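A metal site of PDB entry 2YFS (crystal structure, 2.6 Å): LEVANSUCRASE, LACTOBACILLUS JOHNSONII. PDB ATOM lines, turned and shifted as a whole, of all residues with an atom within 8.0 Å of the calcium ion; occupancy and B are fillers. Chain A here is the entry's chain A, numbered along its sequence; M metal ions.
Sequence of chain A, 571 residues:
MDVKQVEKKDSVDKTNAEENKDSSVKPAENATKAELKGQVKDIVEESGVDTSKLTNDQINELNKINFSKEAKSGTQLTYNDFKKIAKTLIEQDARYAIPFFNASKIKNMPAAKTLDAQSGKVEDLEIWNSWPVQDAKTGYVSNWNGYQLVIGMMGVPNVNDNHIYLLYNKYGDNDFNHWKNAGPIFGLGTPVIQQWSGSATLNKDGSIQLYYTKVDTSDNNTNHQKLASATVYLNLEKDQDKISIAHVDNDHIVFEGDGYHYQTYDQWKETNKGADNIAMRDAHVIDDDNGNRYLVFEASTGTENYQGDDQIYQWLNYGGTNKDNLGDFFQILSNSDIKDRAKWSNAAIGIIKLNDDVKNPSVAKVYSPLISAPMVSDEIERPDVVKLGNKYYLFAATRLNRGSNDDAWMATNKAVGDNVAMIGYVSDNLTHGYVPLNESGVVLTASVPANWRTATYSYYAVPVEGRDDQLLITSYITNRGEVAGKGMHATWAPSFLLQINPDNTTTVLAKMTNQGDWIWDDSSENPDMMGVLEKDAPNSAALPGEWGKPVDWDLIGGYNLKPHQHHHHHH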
ATOM      1  N   GLN A 263      -6.426 -35.422  12.627  1.00  0.00           N
ATOM      2  CA  GLN A 263      -6.524 -36.086  13.917  1.00  0.00           C
ATOM      3  C   GLN A 263      -7.409 -37.329  13.834  1.00  0.00           C
ATOM      4  O   GLN A 263      -8.427 -37.300  13.165  1.00  0.00           O
ATOM      5  CB  GLN A 263      -7.087 -35.121  14.945  1.00  0.00           C
ATOM      6  CG  GLN A 263      -7.080 -35.622  16.375  1.00  0.00           C
ATOM      7  CD  GLN A 263      -7.796 -34.679  17.347  1.00  0.00           C
ATOM      8  OE1 GLN A 263      -8.920 -34.235  17.089  1.00  0.00           O
ATOM      9  NE2 GLN A 263      -7.169 -34.399  18.485  1.00  0.00           N
ATOM     10  N   TRP A 268      -7.450 -38.166  19.701  1.00  0.00           N
ATOM     11  CA  TRP A 268      -8.436 -37.416  20.478  1.00  0.00           C
ATOM     12  C   TRP A 268      -8.644 -38.006  21.860  1.00  0.00           C
ATOM     13  O   TRP A 268      -8.741 -37.267  22.820  1.00  0.00           O
ATOM     14  CB  TRP A 268      -9.779 -37.325  19.745  1.00  0.00           C
ATOM     15  CG  TRP A 268     -10.848 -36.552  20.481  1.00  0.00           C
ATOM     16  CD1 TRP A 268     -11.069 -35.212  20.419  1.00  0.00           C
ATOM     17  CD2 TRP A 268     -11.842 -37.080  21.370  1.00  0.00           C
ATOM     18  NE1 TRP A 268     -12.136 -34.865  21.226  1.00  0.00           N
ATOM     19  CE2 TRP A 268     -12.630 -35.986  21.823  1.00  0.00           C
ATOM     20  CE3 TRP A 268     -12.143 -38.367  21.843  1.00  0.00           C
ATOM     21  CZ2 TRP A 268     -13.696 -36.136  22.713  1.00  0.00           C
ATOM     22  CZ3 TRP A 268     -13.199 -38.523  22.740  1.00  0.00           C
ATOM     23  CH2 TRP A 268     -13.967 -37.407  23.158  1.00  0.00           C
ATOM     24  N   THR A 271      -5.272 -37.039  24.142  1.00  0.00           N
ATOM     25  CA  THR A 271      -5.141 -35.636  24.521  1.00  0.00           C
ATOM     26  C   THR A 271      -6.395 -35.051  25.167  1.00  0.00           C
ATOM     27  O   THR A 271      -6.343 -34.698  26.346  1.00  0.00           O
ATOM     28  CB  THR A 271      -4.586 -34.721  23.376  1.00  0.00           C
ATOM     29  OG1 THR A 271      -5.146 -35.118  22.110  1.00  0.00           O
ATOM     30  CG2 THR A 271      -3.033 -34.801  23.329  1.00  0.00           C
ATOM     31  N   ASN A 272      -7.493 -34.948  24.414  1.00  0.00           N
ATOM     32  CA  ASN A 272      -8.768 -34.414  24.953  1.00  0.00           C
ATOM     33  C   ASN A 272      -8.862 -34.470  26.479  1.00  0.00           C
ATOM     34  O   ASN A 272      -9.032 -35.549  27.076  1.00  0.00           O
ATOM     35  CB  ASN A 272      -9.988 -35.095  24.321  1.00  0.00           C
ATOM     36  CG  ASN A 272     -11.271 -34.875  25.119  1.00  0.00           C
ATOM     37  OD1 ASN A 272     -11.734 -33.749  25.274  1.00  0.00           O
ATOM     38  ND2 ASN A 272     -11.854 -35.955  25.609  1.00  0.00           N
ATOM     39  N   ALA A 275     -12.310 -30.873  27.154  1.00  0.00           N
ATOM     40  CA  ALA A 275     -12.637 -29.658  26.404  1.00  0.00           C
ATOM     41  C   ALA A 275     -12.154 -29.697  24.935  1.00  0.00           C
ATOM     42  O   ALA A 275     -11.413 -28.801  24.489  1.00  0.00           O
ATOM     43  CB  ALA A 275     -12.086 -28.387  27.128  1.00  0.00           C
ATOM     44  N   ASP A 276     -12.575 -30.730  24.207  1.00  0.00           N
ATOM     45  CA  ASP A 276     -12.082 -30.912  22.841  1.00  0.00           C
ATOM     46  C   ASP A 276     -13.126 -31.439  21.873  1.00  0.00           C
ATOM     47  O   ASP A 276     -13.880 -32.379  22.193  1.00  0.00           O
ATOM     48  CB  ASP A 276     -10.820 -31.799  22.817  1.00  0.00           C
ATOM     49  CG  ASP A 276      -9.957 -31.564  21.584  1.00  0.00           C
ATOM     50  OD1 ASP A 276     -10.261 -30.631  20.811  1.00  0.00           O
ATOM     51  OD2 ASP A 276      -8.962 -32.317  21.372  1.00  0.00           O
ATOM     52  N   ASN A 277     -13.154 -30.828  20.698  1.00  0.00           N
ATOM     53  CA  ASN A 277     -14.062 -31.205  19.644  1.00  0.00           C
ATOM     54  C   ASN A 277     -13.435 -32.358  18.881  1.00  0.00           C
ATOM     55  O   ASN A 277     -12.221 -32.452  18.750  1.00  0.00           O
ATOM     56  CB  ASN A 277     -14.310 -30.002  18.721  1.00  0.00           C
ATOM     57  CG  ASN A 277     -15.360 -30.295  17.646  1.00  0.00           C
ATOM     58  OD1 ASN A 277     -16.481 -30.714  17.957  1.00  0.00           O
ATOM     59  ND2 ASN A 277     -14.996 -30.079  16.369  1.00  0.00           N
ATOM     60  N   ILE A 278     -14.284 -33.253  18.388  1.00  0.00           N
ATOM     61  CA  ILE A 278     -13.873 -34.373  17.575  1.00  0.00           C
ATOM     62  C   ILE A 278     -14.652 -34.263  16.264  1.00  0.00           C
ATOM     63  O   ILE A 278     -15.862 -33.988  16.275  1.00  0.00           O
ATOM     64  CB  ILE A 278     -14.055 -35.735  18.358  1.00  0.00           C
ATOM     65  CG1 ILE A 278     -13.523 -36.965  17.589  1.00  0.00           C
ATOM     66  CG2 ILE A 278     -15.463 -35.836  18.983  1.00  0.00           C
ATOM     67  CD1 ILE A 278     -14.379 -37.508  16.430  1.00  0.00           C
ATOM     68  N   ALA A 279     -13.962 -34.420  15.136  1.00  0.00           N
ATOM     69  CA  ALA A 279     -14.572 -34.154  13.837  1.00  0.00           C
ATOM     70  C   ALA A 279     -13.991 -35.017  12.743  1.00  0.00           C
ATOM     71  O   ALA A 279     -12.802 -34.981  12.494  1.00  0.00           O
ATOM     72  CB  ALA A 279     -14.432 -32.692  13.480  1.00  0.00           C
ATOM     73  N   ALA A 299     -12.708 -31.763   9.762  1.00  0.00           N
ATOM     74  CA  ALA A 299     -11.809 -32.544  10.609  1.00  0.00           C
ATOM     75  C   ALA A 299     -11.041 -31.640  11.578  1.00  0.00           C
ATOM     76  O   ALA A 299     -11.357 -30.444  11.754  1.00  0.00           O
ATOM     77  CB  ALA A 299     -10.846 -33.358   9.731  1.00  0.00           C
ATOM     78  N   SER A 300     -10.060 -32.229  12.262  1.00  0.00           N
ATOM     79  CA  SER A 300      -9.081 -31.496  13.027  1.00  0.00           C
ATOM     80  C   SER A 300      -7.711 -31.811  12.467  1.00  0.00           C
ATOM     81  O   SER A 300      -7.485 -32.907  11.936  1.00  0.00           O
ATOM     82  CB  SER A 300      -9.165 -31.890  14.485  1.00  0.00           C
ATOM     83  OG  SER A 300     -10.369 -31.432  15.041  1.00  0.00           O
ATOM     84  N   THR A 301      -6.798 -30.843  12.563  1.00  0.00           N
ATOM     85  CA  THR A 301      -5.432 -31.047  12.083  1.00  0.00           C
ATOM     86  C   THR A 301      -4.775 -32.132  12.935  1.00  0.00           C
ATOM     87  O   THR A 301      -4.969 -32.192  14.149  1.00  0.00           O
ATOM     88  CB  THR A 301      -4.586 -29.755  12.201  1.00  0.00           C
ATOM     89  OG1 THR A 301      -4.551 -29.334  13.573  1.00  0.00           O
ATOM     90  CG2 THR A 301      -5.173 -28.625  11.364  1.00  0.00           C
ATOM     91  N   TYR A 306      -0.446 -29.571  15.108  1.00  0.00           N
ATOM     92  CA  TYR A 306      -1.342 -29.962  16.201  1.00  0.00           C
ATOM     93  C   TYR A 306      -1.693 -28.864  17.197  1.00  0.00           C
ATOM     94  O   TYR A 306      -1.014 -27.846  17.317  1.00  0.00           O
ATOM     95  CB  TYR A 306      -0.719 -31.121  16.957  1.00  0.00           C
ATOM     96  CG  TYR A 306      -1.716 -32.092  17.583  1.00  0.00           C
ATOM     97  CD1 TYR A 306      -2.693 -32.728  16.793  1.00  0.00           C
ATOM     98  CD2 TYR A 306      -1.656 -32.398  18.939  1.00  0.00           C
ATOM     99  CE1 TYR A 306      -3.584 -33.628  17.355  1.00  0.00           C
ATOM    100  CE2 TYR A 306      -2.556 -33.301  19.511  1.00  0.00           C
ATOM    101  CZ  TYR A 306      -3.510 -33.918  18.718  1.00  0.00           C
ATOM    102  OH  TYR A 306      -4.390 -34.811  19.282  1.00  0.00           O
ATOM    103  N   GLN A 307      -2.784 -29.108  17.928  1.00  0.00           N
ATOM    104  CA  GLN A 307      -3.232 -28.234  19.008  1.00  0.00           C
ATOM    105  C   GLN A 307      -2.239 -28.289  20.157  1.00  0.00           C
ATOM    106  O   GLN A 307      -1.414 -29.179  20.233  1.00  0.00           O
ATOM    107  CB  GLN A 307      -4.606 -28.710  19.484  1.00  0.00           C
ATOM    108  CG  GLN A 307      -4.636 -30.202  19.778  1.00  0.00           C
ATOM    109  CD  GLN A 307      -5.995 -30.722  20.191  1.00  0.00           C
ATOM    110  OE1 GLN A 307      -6.903 -30.844  19.376  1.00  0.00           O
ATOM    111  NE2 GLN A 307      -6.135 -31.063  21.468  1.00  0.00           N
ATOM    112  N   GLY A 308      -2.336 -27.318  21.062  1.00  0.00           N
ATOM    113  CA  GLY A 308      -1.502 -27.293  22.232  1.00  0.00           C
ATOM    114  C   GLY A 308      -1.198 -25.892  22.688  1.00  0.00           C
ATOM    115  O   GLY A 308      -1.592 -24.913  22.037  1.00  0.00           O
ATOM    116  N   ARG A 341      -9.355 -22.064  25.156  1.00  0.00           N
ATOM    117  CA  ARG A 341      -9.911 -22.401  23.849  1.00  0.00           C
ATOM    118  C   ARG A 341      -8.853 -22.397  22.757  1.00  0.00           C
ATOM    119  O   ARG A 341      -8.856 -23.267  21.900  1.00  0.00           O
ATOM    120  CB  ARG A 341     -11.052 -21.464  23.474  1.00  0.00           C
ATOM    121  CG  ARG A 341     -12.296 -21.660  24.300  1.00  0.00           C
ATOM    122  CD  ARG A 341     -13.147 -20.426  24.152  1.00  0.00           C
ATOM    123  NE  ARG A 341     -14.508 -20.585  24.653  1.00  0.00           N
ATOM    124  CZ  ARG A 341     -15.560 -20.889  23.899  1.00  0.00           C
ATOM    125  NH1 ARG A 341     -15.421 -21.099  22.596  1.00  0.00           N
ATOM    126  NH2 ARG A 341     -16.762 -20.994  24.457  1.00  0.00           N
ATOM    127  N   ALA A 342      -7.951 -21.417  22.827  1.00  0.00           N
ATOM    128  CA  ALA A 342      -6.822 -21.288  21.903  1.00  0.00           C
ATOM    129  C   ALA A 342      -5.956 -22.534  21.859  1.00  0.00           C
ATOM    130  O   ALA A 342      -5.505 -22.950  20.787  1.00  0.00           O
ATOM    131  CB  ALA A 342      -6.001 -20.095  22.274  1.00  0.00           C
ATOM    132  N   LYS A 343      -5.732 -23.129  23.030  1.00  0.00           N
ATOM    133  CA  LYS A 343      -4.968 -24.357  23.129  1.00  0.00           C
ATOM    134  C   LYS A 343      -5.625 -25.506  22.377  1.00  0.00           C
ATOM    135  O   LYS A 343      -4.944 -26.364  21.833  1.00  0.00           O
ATOM    136  CB  LYS A 343      -4.801 -24.771  24.587  1.00  0.00           C
ATOM    137  CG  LYS A 343      -3.768 -23.985  25.382  1.00  0.00           C
ATOM    138  CD  LYS A 343      -3.552 -24.658  26.748  1.00  0.00           C
ATOM    139  CE  LYS A 343      -3.065 -23.664  27.804  1.00  0.00           C
ATOM    140  NZ  LYS A 343      -2.984 -24.282  29.159  1.00  0.00           N
ATOM    141  N   TRP A 344      -6.955 -25.490  22.329  1.00  0.00           N
ATOM    142  CA  TRP A 344      -7.742 -26.606  21.804  1.00  0.00           C
ATOM    143  C   TRP A 344      -8.244 -26.448  20.367  1.00  0.00           C
ATOM    144  O   TRP A 344      -8.653 -27.428  19.747  1.00  0.00           O
ATOM    145  CB  TRP A 344      -8.889 -26.933  22.765  1.00  0.00           C
ATOM    146  CG  TRP A 344      -8.328 -27.351  24.110  1.00  0.00           C
ATOM    147  CD1 TRP A 344      -8.071 -26.542  25.199  1.00  0.00           C
ATOM    148  CD2 TRP A 344      -7.882 -28.661  24.466  1.00  0.00           C
ATOM    149  NE1 TRP A 344      -7.501 -27.283  26.223  1.00  0.00           N
ATOM    150  CE2 TRP A 344      -7.375 -28.578  25.798  1.00  0.00           C
ATOM    151  CE3 TRP A 344      -7.858 -29.892  23.802  1.00  0.00           C
ATOM    152  CZ2 TRP A 344      -6.857 -29.696  26.481  1.00  0.00           C
ATOM    153  CZ3 TRP A 344      -7.349 -31.008  24.486  1.00  0.00           C
ATOM    154  CH2 TRP A 344      -6.861 -30.906  25.806  1.00  0.00           C
ATOM    155  N   SER A 345      -8.208 -25.230  19.825  1.00  0.00           N
ATOM    156  CA  SER A 345      -8.730 -24.953  18.483  1.00  0.00           C
ATOM    157  C   SER A 345      -7.815 -25.484  17.423  1.00  0.00           C
ATOM    158  O   SER A 345      -6.658 -25.059  17.319  1.00  0.00           O
ATOM    159  CB  SER A 345      -8.853 -23.459  18.263  1.00  0.00           C
ATOM    160  OG  SER A 345      -9.451 -22.841  19.374  1.00  0.00           O
ATOM    161  N   ASN A 346      -8.322 -26.427  16.629  1.00  0.00           N
ATOM    162  CA  ASN A 346      -7.621 -26.824  15.409  1.00  0.00           C
ATOM    163  C   ASN A 346      -8.559 -27.392  14.353  1.00  0.00           C
ATOM    164  O   ASN A 346      -8.304 -28.465  13.776  1.00  0.00           O
ATOM    165  CB  ASN A 346      -6.436 -27.751  15.710  1.00  0.00           C
ATOM    166  CG  ASN A 346      -6.869 -29.124  16.220  1.00  0.00           C
ATOM    167  OD1 ASN A 346      -7.957 -29.271  16.764  1.00  0.00           O
ATOM    168  ND2 ASN A 346      -6.004 -30.136  16.035  1.00  0.00           N
ATOM    169  N   ALA A 347      -9.626 -26.648  14.087  1.00  0.00           N
ATOM    170  CA  ALA A 347     -10.526 -27.027  13.011  1.00  0.00           C
ATOM    171  C   ALA A 347      -9.783 -27.013  11.680  1.00  0.00           C
ATOM    172  O   ALA A 347      -8.818 -26.279  11.511  1.00  0.00           O
ATOM    173  CB  ALA A 347     -11.749 -26.081  12.949  1.00  0.00           C
ATOM    174  N   SER A 377     -10.509 -21.486  15.953  1.00  0.00           N
ATOM    175  CA  SER A 377     -11.809 -22.132  16.026  1.00  0.00           C
ATOM    176  C   SER A 377     -11.640 -23.625  16.113  1.00  0.00           C
ATOM    177  O   SER A 377     -10.700 -24.184  15.539  1.00  0.00           O
ATOM    178  CB  SER A 377     -12.654 -21.801  14.800  1.00  0.00           C
ATOM    179  OG  SER A 377     -13.960 -22.333  14.922  1.00  0.00           O
ATOM    180  N   ASP A 378     -12.568 -24.283  16.801  1.00  0.00           N
ATOM    181  CA  ASP A 378     -12.595 -25.725  16.812  1.00  0.00           C
ATOM    182  C   ASP A 378     -13.753 -26.275  16.015  1.00  0.00           C
ATOM    183  O   ASP A 378     -14.045 -27.466  16.115  1.00  0.00           O
ATOM    184  CB  ASP A 378     -12.596 -26.266  18.236  1.00  0.00           C
ATOM    185  CG  ASP A 378     -11.587 -27.438  18.421  1.00  0.00           C
ATOM    186  OD1 ASP A 378     -10.728 -27.667  17.514  1.00  0.00           O
ATOM    187  OD2 ASP A 378     -11.651 -28.144  19.475  1.00  0.00           O
ATOM    188  N   GLU A 379     -14.407 -25.447  15.196  1.00  0.00           N
ATOM    189  CA  GLU A 379     -15.516 -25.937  14.389  1.00  0.00           C
ATOM    190  C   GLU A 379     -15.848 -25.167  13.114  1.00  0.00           C
ATOM    191  O   GLU A 379     -16.456 -24.096  13.156  1.00  0.00           O
ATOM    192  CB  GLU A 379     -16.781 -26.096  15.242  1.00  0.00           C
ATOM    193  CG  GLU A 379     -17.728 -27.163  14.682  1.00  0.00           C
ATOM    194  CD  GLU A 379     -18.928 -27.430  15.551  1.00  0.00           C
ATOM    195  OE1 GLU A 379     -19.795 -26.517  15.682  1.00  0.00           O
ATOM    196  OE2 GLU A 379     -19.023 -28.567  16.087  1.00  0.00           O
HETATM  197 CA    CA M   1      -9.045 -29.596  18.842  1.00  0.00          CA
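The calcium ion is bound by the side-chain amide oxygen of Asn 346 (2.4 Å), the backbone carbonyl oxygen of Trp 344 (2.4 Å), the side-chain carboxylate of Asp 276 (2.5 Å), the side-chain amide oxygen of Gln 307 (2.5 Å) and the side-chain carboxylate of Asp 378 (2.9 Å).
The calcium ion has five donor atoms within binding distance.
Slightly farther from the calcium ion lies the side-chain carboxylate (OD2) of Asp 378 (3.0 Å).
The side-chain hydroxyl of Thr 301 sits at hydrogen-bond distance from the side-chain amide nitrogen of Asn 346, at 3.0 Å.
N of Asn 346 lies within hydrogen-bond range of O of Ser 377, at 3.4 Å.
The backbone NH (N) of Asp 276 sits close to the side-chain amide oxygen (OD1) of Asn 272 (3.3 Å).
ND2 of Asn 277 sits at hydrogen-bond distance from O of Asp 378.
NE1 of Trp 268 sits at hydrogen-bond distance from O of Asp 276 (3.2 Å).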
